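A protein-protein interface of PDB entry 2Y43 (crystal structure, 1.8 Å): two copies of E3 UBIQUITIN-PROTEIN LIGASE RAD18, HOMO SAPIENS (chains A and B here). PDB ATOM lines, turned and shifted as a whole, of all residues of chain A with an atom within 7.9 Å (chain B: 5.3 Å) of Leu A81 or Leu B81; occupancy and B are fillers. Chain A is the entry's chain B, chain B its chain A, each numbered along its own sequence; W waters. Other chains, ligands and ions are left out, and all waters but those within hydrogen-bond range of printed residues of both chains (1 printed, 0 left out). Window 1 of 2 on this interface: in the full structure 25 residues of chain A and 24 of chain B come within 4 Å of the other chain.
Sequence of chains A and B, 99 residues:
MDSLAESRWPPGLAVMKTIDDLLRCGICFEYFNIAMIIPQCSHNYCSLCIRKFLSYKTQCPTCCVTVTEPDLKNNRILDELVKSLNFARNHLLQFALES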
ATOM      1  N   THR A  18      23.949 -16.519  -3.906  1.00  0.00           N
ATOM      2  CA  THR A  18      23.604 -15.145  -4.282  1.00  0.00           C
ATOM      3  C   THR A  18      22.083 -14.926  -4.269  1.00  0.00           C
ATOM      4  O   THR A  18      21.578 -13.931  -3.734  1.00  0.00           O
ATOM      5  CB  THR A  18      24.188 -14.785  -5.672  1.00  0.00           C
ATOM      6  OG1 THR A  18      25.602 -15.024  -5.683  1.00  0.00           O
ATOM      7  CG2 THR A  18      23.923 -13.319  -6.000  1.00  0.00           C
ATOM      8  N   ILE A  19      21.357 -15.878  -4.841  1.00  0.00           N
ATOM      9  CA  ILE A  19      19.917 -15.808  -4.908  1.00  0.00           C
ATOM     10  C   ILE A  19      19.305 -15.974  -3.509  1.00  0.00           C
ATOM     11  O   ILE A  19      18.427 -15.201  -3.110  1.00  0.00           O
ATOM     12  CB  ILE A  19      19.370 -16.845  -5.914  1.00  0.00           C
ATOM     13  CG1 ILE A  19      19.918 -16.503  -7.311  1.00  0.00           C
ATOM     14  CG2 ILE A  19      17.840 -16.838  -5.898  1.00  0.00           C
ATOM     15  CD1 ILE A  19      20.083 -17.691  -8.205  1.00  0.00           C
ATOM     16  N   ASP A  20      19.804 -16.963  -2.763  1.00  0.00           N
ATOM     17  CA  ASP A  20      19.366 -17.180  -1.385  1.00  0.00           C
ATOM     18  C   ASP A  20      19.522 -15.929  -0.500  1.00  0.00           C
ATOM     19  O   ASP A  20      18.610 -15.582   0.281  1.00  0.00           O
ATOM     20  CB  ASP A  20      20.134 -18.348  -0.783  1.00  0.00           C
ATOM     21  CG  ASP A  20      19.351 -19.053   0.293  1.00  0.00           C
ATOM     22  OD1 ASP A  20      19.387 -18.606   1.463  1.00  0.00           O
ATOM     23  OD2 ASP A  20      18.692 -20.052  -0.040  1.00  0.00           O
ATOM     24  N   ASP A  21      20.665 -15.261  -0.644  1.00  0.00           N
ATOM     25  CA  ASP A  21      20.968 -14.031   0.095  1.00  0.00           C
ATOM     26  C   ASP A  21      20.009 -12.892  -0.246  1.00  0.00           C
ATOM     27  O   ASP A  21      19.595 -12.126   0.631  1.00  0.00           O
ATOM     28  CB  ASP A  21      22.410 -13.576  -0.171  1.00  0.00           C
ATOM     29  CG  ASP A  21      23.461 -14.402   0.585  1.00  0.00           C
ATOM     30  OD1 ASP A  21      23.130 -15.125   1.550  1.00  0.00           O
ATOM     31  OD2 ASP A  21      24.648 -14.283   0.236  1.00  0.00           O
ATOM     32  N   LEU A  22      19.664 -12.762  -1.524  1.00  0.00           N
ATOM     33  CA  LEU A  22      18.719 -11.711  -1.960  1.00  0.00           C
ATOM     34  C   LEU A  22      17.327 -11.853  -1.379  1.00  0.00           C
ATOM     35  O   LEU A  22      16.587 -10.877  -1.302  1.00  0.00           O
ATOM     36  CB  LEU A  22      18.625 -11.656  -3.491  1.00  0.00           C
ATOM     37  CG  LEU A  22      19.869 -11.038  -4.158  1.00  0.00           C
ATOM     38  CD1 LEU A  22      19.869 -11.322  -5.643  1.00  0.00           C
ATOM     39  CD2 LEU A  22      19.920  -9.527  -3.904  1.00  0.00           C
ATOM     40  N   LEU A  23      16.977 -13.064  -0.965  1.00  0.00           N
ATOM     41  CA  LEU A  23      15.636 -13.328  -0.500  1.00  0.00           C
ATOM     42  C   LEU A  23      15.556 -13.298   1.010  1.00  0.00           C
ATOM     43  O   LEU A  23      14.566 -13.735   1.569  1.00  0.00           O
ATOM     44  CB  LEU A  23      15.122 -14.668  -1.054  1.00  0.00           C
ATOM     45  CG  LEU A  23      14.904 -14.752  -2.567  1.00  0.00           C
ATOM     46  CD1 LEU A  23      14.385 -16.131  -2.958  1.00  0.00           C
ATOM     47  CD2 LEU A  23      13.938 -13.693  -3.047  1.00  0.00           C
ATOM     48  N   TYR A  31      14.522 -15.562   5.608  1.00  0.00           N
ATOM     49  CA  TYR A  31      13.767 -15.333   4.375  1.00  0.00           C
ATOM     50  C   TYR A  31      12.622 -14.370   4.665  1.00  0.00           C
ATOM     51  O   TYR A  31      11.952 -14.501   5.713  1.00  0.00           O
ATOM     52  CB  TYR A  31      13.177 -16.640   3.850  1.00  0.00           C
ATOM     53  CG  TYR A  31      14.216 -17.607   3.333  1.00  0.00           C
ATOM     54  CD1 TYR A  31      14.958 -17.311   2.188  1.00  0.00           C
ATOM     55  CD2 TYR A  31      14.443 -18.817   3.985  1.00  0.00           C
ATOM     56  CE1 TYR A  31      15.933 -18.196   1.715  1.00  0.00           C
ATOM     57  CE2 TYR A  31      15.400 -19.718   3.521  1.00  0.00           C
ATOM     58  CZ  TYR A  31      16.137 -19.403   2.380  1.00  0.00           C
ATOM     59  OH  TYR A  31      17.092 -20.299   1.930  1.00  0.00           O
ATOM     60  N   PHE A  32      12.394 -13.444   3.731  1.00  0.00           N
ATOM     61  CA  PHE A  32      11.268 -12.501   3.824  1.00  0.00           C
ATOM     62  C   PHE A  32       9.990 -13.208   4.229  1.00  0.00           C
ATOM     63  O   PHE A  32       9.569 -14.212   3.625  1.00  0.00           O
ATOM     64  CB  PHE A  32      11.019 -11.755   2.521  1.00  0.00           C
ATOM     65  CG  PHE A  32      12.121 -10.812   2.128  1.00  0.00           C
ATOM     66  CD1 PHE A  32      12.430  -9.697   2.912  1.00  0.00           C
ATOM     67  CD2 PHE A  32      12.849 -11.042   0.968  1.00  0.00           C
ATOM     68  CE1 PHE A  32      13.466  -8.822   2.539  1.00  0.00           C
ATOM     69  CE2 PHE A  32      13.887 -10.175   0.584  1.00  0.00           C
ATOM     70  CZ  PHE A  32      14.193  -9.062   1.380  1.00  0.00           C
ATOM     71  N   ASN A  44      13.476  -3.657   1.064  1.00  0.00           N
ATOM     72  CA  ASN A  44      12.447  -4.640   1.426  1.00  0.00           C
ATOM     73  C   ASN A  44      12.772  -5.276   2.757  1.00  0.00           C
ATOM     74  O   ASN A  44      13.949  -5.536   3.052  1.00  0.00           O
ATOM     75  CB  ASN A  44      12.369  -5.761   0.363  1.00  0.00           C
ATOM     76  CG  ASN A  44      11.981  -5.241  -1.012  1.00  0.00           C
ATOM     77  OD1 ASN A  44      10.820  -4.908  -1.259  1.00  0.00           O
ATOM     78  ND2 ASN A  44      12.955  -5.179  -1.915  1.00  0.00           N
ATOM     79  N   ASN A  75       5.289  -6.504  -1.093  1.00  0.00           N
ATOM     80  CA  ASN A  75       6.047  -6.924  -2.275  1.00  0.00           C
ATOM     81  C   ASN A  75       5.824  -8.432  -2.464  1.00  0.00           C
ATOM     82  O   ASN A  75       6.668  -9.252  -2.126  1.00  0.00           O
ATOM     83  CB  ASN A  75       7.538  -6.549  -2.134  1.00  0.00           C
ATOM     84  CG  ASN A  75       8.260  -6.485  -3.477  1.00  0.00           C
ATOM     85  OD1 ASN A  75       7.734  -6.945  -4.492  1.00  0.00           O
ATOM     86  ND2 ASN A  75       9.475  -5.918  -3.480  1.00  0.00           N
ATOM     87  N   ARG A  76       4.664  -8.776  -3.018  1.00  0.00           N
ATOM     88  CA  ARG A  76       4.160 -10.150  -2.984  1.00  0.00           C
ATOM     89  C   ARG A  76       5.032 -11.139  -3.727  1.00  0.00           C
ATOM     90  O   ARG A  76       5.112 -12.310  -3.330  1.00  0.00           O
ATOM     91  CB  ARG A  76       2.711 -10.216  -3.481  1.00  0.00           C
ATOM     92  CG  ARG A  76       1.768  -9.481  -2.520  1.00  0.00           C
ATOM     93  CD  ARG A  76       0.286  -9.548  -2.895  1.00  0.00           C
ATOM     94  NE  ARG A  76      -0.498  -8.606  -2.076  1.00  0.00           N
ATOM     95  CZ  ARG A  76      -0.771  -8.771  -0.777  1.00  0.00           C
ATOM     96  NH1 ARG A  76      -0.326  -9.841  -0.120  1.00  0.00           N
ATOM     97  NH2 ARG A  76      -1.491  -7.857  -0.120  1.00  0.00           N
ATOM     98  N   ILE A  77       5.690 -10.667  -4.784  1.00  0.00           N
ATOM     99  CA  ILE A  77       6.530 -11.558  -5.606  1.00  0.00           C
ATOM    100  C   ILE A  77       7.676 -12.167  -4.784  1.00  0.00           C
ATOM    101  O   ILE A  77       8.102 -13.285  -5.059  1.00  0.00           O
ATOM    102  CB  ILE A  77       7.100 -10.835  -6.870  1.00  0.00           C
ATOM    103  CG1 ILE A  77       7.570 -11.874  -7.915  1.00  0.00           C
ATOM    104  CG2 ILE A  77       8.195  -9.828  -6.479  1.00  0.00           C
ATOM    105  CD1 ILE A  77       8.091 -11.260  -9.232  1.00  0.00           C
ATOM    106  N   LEU A  78       8.143 -11.448  -3.761  1.00  0.00           N
ATOM    107  CA  LEU A  78       9.209 -11.972  -2.889  1.00  0.00           C
ATOM    108  C   LEU A  78       8.716 -13.145  -2.048  1.00  0.00           C
ATOM    109  O   LEU A  78       9.474 -14.097  -1.788  1.00  0.00           O
ATOM    110  CB  LEU A  78       9.762 -10.875  -1.975  1.00  0.00           C
ATOM    111  CG  LEU A  78      10.498  -9.767  -2.721  1.00  0.00           C
ATOM    112  CD1 LEU A  78      11.064  -8.742  -1.722  1.00  0.00           C
ATOM    113  CD2 LEU A  78      11.653 -10.335  -3.565  1.00  0.00           C
ATOM    114  N   ASP A  79       7.457 -13.078  -1.624  1.00  0.00           N
ATOM    115  CA  ASP A  79       6.846 -14.206  -0.891  1.00  0.00           C
ATOM    116  C   ASP A  79       6.774 -15.443  -1.800  1.00  0.00           C
ATOM    117  O   ASP A  79       7.015 -16.581  -1.352  1.00  0.00           O
ATOM    118  CB  ASP A  79       5.423 -13.859  -0.391  1.00  0.00           C
ATOM    119  CG  ASP A  79       5.404 -12.654   0.559  1.00  0.00           C
ATOM    120  OD1 ASP A  79       6.367 -12.482   1.337  1.00  0.00           O
ATOM    121  OD2 ASP A  79       4.409 -11.887   0.537  1.00  0.00           O
ATOM    122  N   GLU A  80       6.396 -15.219  -3.057  1.00  0.00           N
ATOM    123  CA  GLU A  80       6.314 -16.296  -4.039  1.00  0.00           C
ATOM    124  C   GLU A  80       7.715 -16.875  -4.296  1.00  0.00           C
ATOM    125  O   GLU A  80       7.879 -18.085  -4.415  1.00  0.00           O
ATOM    126  CB  GLU A  80       5.709 -15.787  -5.354  1.00  0.00           C
ATOM    127  CG  GLU A  80       4.221 -15.340  -5.280  1.00  0.00           C
ATOM    128  CD  GLU A  80       3.207 -16.483  -5.301  1.00  0.00           C
ATOM    129  OE1 GLU A  80       3.586 -17.662  -5.485  1.00  0.00           O
ATOM    130  OE2 GLU A  80       1.992 -16.198  -5.135  1.00  0.00           O
ATOM    131  N   LEU A  81       8.711 -16.003  -4.386  1.00  0.00           N
ATOM    132  CA  LEU A  81      10.074 -16.460  -4.651  1.00  0.00           C
ATOM    133  C   LEU A  81      10.646 -17.262  -3.488  1.00  0.00           C
ATOM    134  O   LEU A  81      11.285 -18.295  -3.700  1.00  0.00           O
ATOM    135  CB  LEU A  81      10.991 -15.295  -5.016  1.00  0.00           C
ATOM    136  CG  LEU A  81      10.768 -14.732  -6.431  1.00  0.00           C
ATOM    137  CD1 LEU A  81      11.266 -13.275  -6.524  1.00  0.00           C
ATOM    138  CD2 LEU A  81      11.454 -15.612  -7.485  1.00  0.00           C
ATOM    139  N   VAL A  82      10.389 -16.800  -2.265  1.00  0.00           N
ATOM    140  CA  VAL A  82      10.815 -17.533  -1.056  1.00  0.00           C
ATOM    141  C   VAL A  82      10.226 -18.924  -1.012  1.00  0.00           C
ATOM    142  O   VAL A  82      10.949 -19.912  -0.758  1.00  0.00           O
ATOM    143  CB  VAL A  82      10.460 -16.760   0.269  1.00  0.00           C
ATOM    144  CG1 VAL A  82      10.585 -17.667   1.495  1.00  0.00           C
ATOM    145  CG2 VAL A  82      11.351 -15.523   0.420  1.00  0.00           C
ATOM    146  N   LYS A  83       8.916 -19.018  -1.268  1.00  0.00           N
ATOM    147  CA  LYS A  83       8.247 -20.306  -1.298  1.00  0.00           C
ATOM    148  C   LYS A  83       8.852 -21.206  -2.372  1.00  0.00           C
ATOM    149  O   LYS A  83       9.147 -22.382  -2.129  1.00  0.00           O
ATOM    150  CB  LYS A  83       6.744 -20.135  -1.541  1.00  0.00           C
ATOM    151  CG  LYS A  83       5.933 -21.431  -1.391  1.00  0.00           C
ATOM    152  CD  LYS A  83       5.500 -21.651   0.057  1.00  0.00           C
ATOM    153  CE  LYS A  83       4.279 -22.584   0.194  1.00  0.00           C
ATOM    154  NZ  LYS A  83       4.487 -23.989  -0.271  1.00  0.00           N
ATOM    155  N   SER A  84       9.047 -20.652  -3.562  1.00  0.00           N
ATOM    156  CA  SER A  84       9.499 -21.477  -4.687  1.00  0.00           C
ATOM    157  C   SER A  84      10.946 -21.905  -4.510  1.00  0.00           C
ATOM    158  O   SER A  84      11.288 -23.040  -4.807  1.00  0.00           O
ATOM    159  CB  SER A  84       9.272 -20.747  -6.008  1.00  0.00           C
ATOM    160  OG  SER A  84       7.871 -20.676  -6.242  1.00  0.00           O
ATOM    161  N   LEU A  85      11.783 -21.009  -3.994  1.00  0.00           N
ATOM    162  CA  LEU A  85      13.175 -21.370  -3.714  1.00  0.00           C
ATOM    163  C   LEU A  85      13.323 -22.451  -2.648  1.00  0.00           C
ATOM    164  O   LEU A  85      14.128 -23.373  -2.806  1.00  0.00           O
ATOM    165  CB  LEU A  85      14.020 -20.146  -3.357  1.00  0.00           C
ATOM    166  CG  LEU A  85      15.538 -20.341  -3.590  1.00  0.00           C
ATOM    167  CD1 LEU A  85      15.916 -20.402  -5.064  1.00  0.00           C
ATOM    168  CD2 LEU A  85      16.327 -19.229  -2.907  1.00  0.00           C
ATOM    169  N   ASN A  86      12.560 -22.337  -1.562  1.00  0.00           N
ATOM    170  CA  ASN A  86      12.513 -23.405  -0.546  1.00  0.00           C
ATOM    171  C   ASN A  86      12.096 -24.744  -1.163  1.00  0.00           C
ATOM    172  O   ASN A  86      12.721 -25.797  -0.887  1.00  0.00           O
ATOM    173  CB  ASN A  86      11.551 -23.038   0.591  1.00  0.00           C
ATOM    174  CG  ASN A  86      11.399 -24.165   1.621  1.00  0.00           C
ATOM    175  OD1 ASN A  86      12.324 -24.450   2.384  1.00  0.00           O
ATOM    176  ND2 ASN A  86      10.235 -24.819   1.634  1.00  0.00           N
ATOM    177  N   PHE A  87      11.038 -24.723  -1.980  1.00  0.00           N
ATOM    178  CA  PHE A  87      10.584 -25.948  -2.639  1.00  0.00           C
ATOM    179  C   PHE A  87      11.705 -26.519  -3.502  1.00  0.00           C
ATOM    180  O   PHE A  87      12.017 -27.714  -3.412  1.00  0.00           O
ATOM    181  CB  PHE A  87       9.331 -25.731  -3.497  1.00  0.00           C
ATOM    182  CG  PHE A  87       8.866 -26.987  -4.195  1.00  0.00           C
ATOM    183  CD1 PHE A  87       9.381 -27.340  -5.443  1.00  0.00           C
ATOM    184  CD2 PHE A  87       7.945 -27.836  -3.587  1.00  0.00           C
ATOM    185  CE1 PHE A  87       8.974 -28.510  -6.081  1.00  0.00           C
ATOM    186  CE2 PHE A  87       7.526 -29.015  -4.218  1.00  0.00           C
ATOM    187  CZ  PHE A  87       8.037 -29.350  -5.467  1.00  0.00           C
ATOM    188  N   ALA A  88      12.299 -25.662  -4.339  1.00  0.00           N
ATOM    189  CA  ALA A  88      13.382 -26.094  -5.239  1.00  0.00           C
ATOM    190  C   ALA A  88      14.524 -26.726  -4.454  1.00  0.00           C
ATOM    191  O   ALA A  88      14.976 -27.816  -4.782  1.00  0.00           O
ATOM    192  CB  ALA A  88      13.896 -24.914  -6.063  1.00  0.00           C
ATOM    193  N   ILE B  19      11.264 -20.751 -10.680  1.00  0.00           N
ATOM    194  CA  ILE B  19      11.854 -19.449 -10.367  1.00  0.00           C
ATOM    195  C   ILE B  19      11.912 -18.594 -11.642  1.00  0.00           C
ATOM    196  O   ILE B  19      11.594 -17.402 -11.610  1.00  0.00           O
ATOM    197  CB  ILE B  19      13.286 -19.582  -9.742  1.00  0.00           C
ATOM    198  CG1 ILE B  19      13.351 -20.689  -8.673  1.00  0.00           C
ATOM    199  CG2 ILE B  19      13.779 -18.229  -9.195  1.00  0.00           C
ATOM    200  CD1 ILE B  19      12.475 -20.480  -7.453  1.00  0.00           C
ATOM    201  N   LEU B  22       8.589 -16.898 -12.276  1.00  0.00           N
ATOM    202  CA  LEU B  22       8.270 -15.766 -11.414  1.00  0.00           C
ATOM    203  C   LEU B  22       9.004 -14.491 -11.831  1.00  0.00           C
ATOM    204  O   LEU B  22       8.580 -13.388 -11.483  1.00  0.00           O
ATOM    205  CB  LEU B  22       8.560 -16.082  -9.940  1.00  0.00           C
ATOM    206  CG  LEU B  22       7.620 -17.073  -9.264  1.00  0.00           C
ATOM    207  CD1 LEU B  22       8.214 -17.541  -7.929  1.00  0.00           C
ATOM    208  CD2 LEU B  22       6.207 -16.477  -9.111  1.00  0.00           C
ATOM    209  N   LEU B  23      10.097 -14.630 -12.572  1.00  0.00           N
ATOM    210  CA  LEU B  23      10.870 -13.447 -12.973  1.00  0.00           C
ATOM    211  C   LEU B  23      10.532 -12.992 -14.399  1.00  0.00           C
ATOM    212  O   LEU B  23      11.269 -12.210 -14.981  1.00  0.00           O
ATOM    213  CB  LEU B  23      12.387 -13.694 -12.807  1.00  0.00           C
ATOM    214  CG  LEU B  23      12.878 -13.894 -11.365  1.00  0.00           C
ATOM    215  CD1 LEU B  23      14.405 -14.078 -11.317  1.00  0.00           C
ATOM    216  CD2 LEU B  23      12.465 -12.720 -10.475  1.00  0.00           C
ATOM    217  N   ILE B  77      15.029  -4.969  -6.439  1.00  0.00           N
ATOM    218  CA  ILE B  77      15.401  -6.354  -6.104  1.00  0.00           C
ATOM    219  C   ILE B  77      15.181  -7.342  -7.256  1.00  0.00           C
ATOM    220  O   ILE B  77      15.979  -8.286  -7.441  1.00  0.00           O
ATOM    221  CB  ILE B  77      14.710  -6.845  -4.787  1.00  0.00           C
ATOM    222  CG1 ILE B  77      15.481  -8.027  -4.172  1.00  0.00           C
ATOM    223  CG2 ILE B  77      13.194  -7.147  -5.030  1.00  0.00           C
ATOM    224  CD1 ILE B  77      14.982  -8.445  -2.761  1.00  0.00           C
ATOM    225  N   LEU B  78      14.142  -7.122  -8.062  1.00  0.00           N
ATOM    226  CA  LEU B  78      13.882  -8.035  -9.188  1.00  0.00           C
ATOM    227  C   LEU B  78      14.998  -8.009 -10.242  1.00  0.00           C
ATOM    228  O   LEU B  78      15.336  -9.058 -10.814  1.00  0.00           O
ATOM    229  CB  LEU B  78      12.524  -7.745  -9.839  1.00  0.00           C
ATOM    230  CG  LEU B  78      11.326  -8.041  -8.935  1.00  0.00           C
ATOM    231  CD1 LEU B  78       9.989  -7.699  -9.651  1.00  0.00           C
ATOM    232  CD2 LEU B  78      11.343  -9.531  -8.473  1.00  0.00           C
ATOM    233  N   ASP B  79      15.548  -6.827 -10.506  1.00  0.00           N
ATOM    234  CA  ASP B  79      16.641  -6.699 -11.482  1.00  0.00           C
ATOM    235  C   ASP B  79      17.880  -7.458 -10.989  1.00  0.00           C
ATOM    236  O   ASP B  79      18.586  -8.090 -11.785  1.00  0.00           O
ATOM    237  CB  ASP B  79      17.021  -5.233 -11.714  1.00  0.00           C
ATOM    238  CG  ASP B  79      15.842  -4.356 -12.115  1.00  0.00           C
ATOM    239  OD1 ASP B  79      14.867  -4.861 -12.712  1.00  0.00           O
ATOM    240  OD2 ASP B  79      15.910  -3.126 -11.825  1.00  0.00           O
ATOM    241  N   GLU B  80      18.157  -7.364  -9.682  1.00  0.00           N
ATOM    242  CA  GLU B  80      19.279  -8.093  -9.078  1.00  0.00           C
ATOM    243  C   GLU B  80      19.054  -9.605  -9.144  1.00  0.00           C
ATOM    244  O   GLU B  80      19.978 -10.366  -9.400  1.00  0.00           O
ATOM    245  CB  GLU B  80      19.482  -7.663  -7.617  1.00  0.00           C
ATOM    246  CG  GLU B  80      19.955  -6.219  -7.465  1.00  0.00           C
ATOM    247  CD  GLU B  80      21.319  -5.962  -8.115  1.00  0.00           C
ATOM    248  OE1 GLU B  80      22.222  -6.831  -8.010  1.00  0.00           O
ATOM    249  OE2 GLU B  80      21.494  -4.879  -8.728  1.00  0.00           O
ATOM    250  N   LEU B  81      17.812 -10.018  -8.920  1.00  0.00           N
ATOM    251  CA  LEU B  81      17.449 -11.447  -8.958  1.00  0.00           C
ATOM    252  C   LEU B  81      17.605 -11.988 -10.366  1.00  0.00           C
ATOM    253  O   LEU B  81      18.184 -13.078 -10.567  1.00  0.00           O
ATOM    254  CB  LEU B  81      16.011 -11.646  -8.445  1.00  0.00           C
ATOM    255  CG  LEU B  81      15.907 -11.635  -6.903  1.00  0.00           C
ATOM    256  CD1 LEU B  81      14.472 -11.305  -6.430  1.00  0.00           C
ATOM    257  CD2 LEU B  81      16.430 -12.945  -6.291  1.00  0.00           C
ATOM    258  N   VAL B  82      17.123 -11.215 -11.341  1.00  0.00           N
ATOM    259  CA  VAL B  82      17.283 -11.588 -12.761  1.00  0.00           C
ATOM    260  C   VAL B  82      18.764 -11.753 -13.111  1.00  0.00           C
ATOM    261  O   VAL B  82      19.163 -12.764 -13.714  1.00  0.00           O
ATOM    262  CB  VAL B  82      16.585 -10.586 -13.730  1.00  0.00           C
ATOM    263  CG1 VAL B  82      17.038 -10.837 -15.197  1.00  0.00           C
ATOM    264  CG2 VAL B  82      15.037 -10.701 -13.603  1.00  0.00           C
ATOM    265  N   LYS B  83      19.577 -10.772 -12.726  1.00  0.00           N
ATOM    266  CA  LYS B  83      21.018 -10.804 -13.015  1.00  0.00           C
ATOM    267  C   LYS B  83      21.668 -12.035 -12.398  1.00  0.00           C
ATOM    268  O   LYS B  83      22.475 -12.710 -13.051  1.00  0.00           O
ATOM    269  CB  LYS B  83      21.704  -9.525 -12.502  1.00  0.00           C
ATOM    270  CG  LYS B  83      23.216  -9.417 -12.794  1.00  0.00           C
ATOM    271  CD  LYS B  83      23.810  -8.160 -12.123  1.00  0.00           C
ATOM    272  CE  LYS B  83      24.980  -7.554 -12.926  1.00  0.00           C
ATOM    273  NZ  LYS B  83      26.163  -8.462 -13.114  1.00  0.00           N
ATOM    274  N   SER B  84      21.312 -12.323 -11.148  1.00  0.00           N
ATOM    275  CA  SER B  84      21.935 -13.420 -10.402  1.00  0.00           C
ATOM    276  C   SER B  84      21.515 -14.769 -10.946  1.00  0.00           C
ATOM    277  O   SER B  84      22.350 -15.672 -11.080  1.00  0.00           O
ATOM    278  CB  SER B  84      21.604 -13.313  -8.914  1.00  0.00           C
ATOM    279  OG  SER B  84      22.152 -12.108  -8.402  1.00  0.00           O
ATOM    280  N   LEU B  85      20.226 -14.897 -11.264  1.00  0.00           N
ATOM    281  CA  LEU B  85      19.695 -16.148 -11.779  1.00  0.00           C
ATOM    282  C   LEU B  85      20.269 -16.427 -13.172  1.00  0.00           C
ATOM    283  O   LEU B  85      20.587 -17.583 -13.498  1.00  0.00           O
ATOM    284  CB  LEU B  85      18.154 -16.153 -11.784  1.00  0.00           C
ATOM    285  CG  LEU B  85      17.495 -17.538 -11.945  1.00  0.00           C
ATOM    286  CD1 LEU B  85      17.825 -18.483 -10.776  1.00  0.00           C
ATOM    287  CD2 LEU B  85      15.988 -17.383 -12.102  1.00  0.00           C
ATOM    288  N   ASN B  86      20.426 -15.377 -13.982  1.00  0.00           N
ATOM    289  CA  ASN B  86      21.077 -15.521 -15.301  1.00  0.00           C
ATOM    290  C   ASN B  86      22.498 -16.081 -15.149  1.00  0.00           C
ATOM    291  O   ASN B  86      22.902 -17.005 -15.876  1.00  0.00           O
ATOM    292  CB  ASN B  86      21.135 -14.183 -16.049  1.00  0.00           C
ATOM    293  CG  ASN B  86      19.801 -13.779 -16.666  1.00  0.00           C
ATOM    294  OD1 ASN B  86      18.836 -14.548 -16.680  1.00  0.00           O
ATOM    295  ND2 ASN B  86      19.745 -12.552 -17.175  1.00  0.00           N
HETATM  296  O   HOH W   1      12.893  -3.937  -4.548  1.00  0.00           O
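OG of Ser B84 lies within hydrogen-bond range of O of Glu B80 (3.0 Å).
The backbone NH of Phe A32 lies within hydrogen-bond range of the backbone carbonyl oxygen of Leu A23 (3.1 Å).
The side-chain amide nitrogen of Asn A75 is in hydrogen-bond range of the side-chain amide oxygen of Asn A44 (2.8 Å).
OG of Ser A84 sits at hydrogen-bond distance from O of Glu A80.
CG2 of Thr A18 touches OG of Ser B84 (3.2 Å).
Leu B85 touches Ile A19.
Ile B77 touches Leu A22.
CE2 of Phe A32 touches CD1 of Ile B77, 3.9 Å away.
Asn A44 touches Ile B77.
Ile A77 touches Leu B22 (CD1 to O, 3.1 Å).
Ile A77 touches Leu B78 (CG2 to CD2, 3.7 Å).
CD1 of Leu A81 touches CD1 of Leu B81, 3.8 Å away.
Ser A84 touches Leu B22 (OG to CD1, 3.6 Å).
Leu A85 touches Ile B19 (N to CD1, 3.6 Å).
Ile A19 touches Leu B85, and with the chains exchanged Leu A85 touches Ile B19.
Leu A22 touches Glu B80, and with the chains exchanged Glu A80 touches Leu B22.
Leu A22 touches Ser B84, and with the chains exchanged Ser A84 touches Leu B22.
Leu A81 touches Ile B19, but with the chains exchanged Ile A19 does not touch Leu B81 (4.2 Å).
Of the 19 pairs that touch across the chains among the printed residues, 15 have their exchanged pair printed and touching as well.
Of the 23 printed residues of chain A, 11 touch a printed residue of chain B.
Hydrophobic or aromatic side chains of chain A within 4 Å of the printed part of chain B: Ile A19, Leu A22, Phe A32, Ile A77, Leu A78 and Leu A81.
Printed residues of chain B that touch a printed residue of chain A: Ile B19, Leu B22, Ile B77, Leu B78, Glu B80, Leu B81, Ser B84 and Leu B85.
Among the printed residues, no Asp or Glu carboxylate lies within 4 Å of a Lys or Arg side-chain nitrogen of the other chain.
Water W1 lies within hydrogen-bond range of the side-chain amide nitrogen (ND2) of Asn A44 (2.9 Å) and the backbone NH (N) of Ile B77 (3.0 Å).
Of chain B, only Ile B19 (3.9 Å), Leu B22 (3.8 Å) and Leu B81 (3.8 Å) come within 4 Å of Leu A81.
Leu B81 touches two residues of chain A.
Printed residues of chain A within 4 Å of Leu B78: Ile A77.
Printed residues of chain A within 4 Å of Ile B19: Leu A81, Ser A84 and Leu A85.
Of the printed residues of chain B, Ser A84 touches Ile B19 (3.5 Å) and Leu B22 (3.6 Å).
Printed residues of chain B within 4 Å of Glu A80: Leu B22 (3.6 Å).
Of the printed residues of chain B, Ile A19 touches Ser B84 and Leu B85.
Leu B23 touches none of the printed residues of chain A.
The nearest printed residue of chain B that does not touch Leu A22 is Val B82 (6.3 Å).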
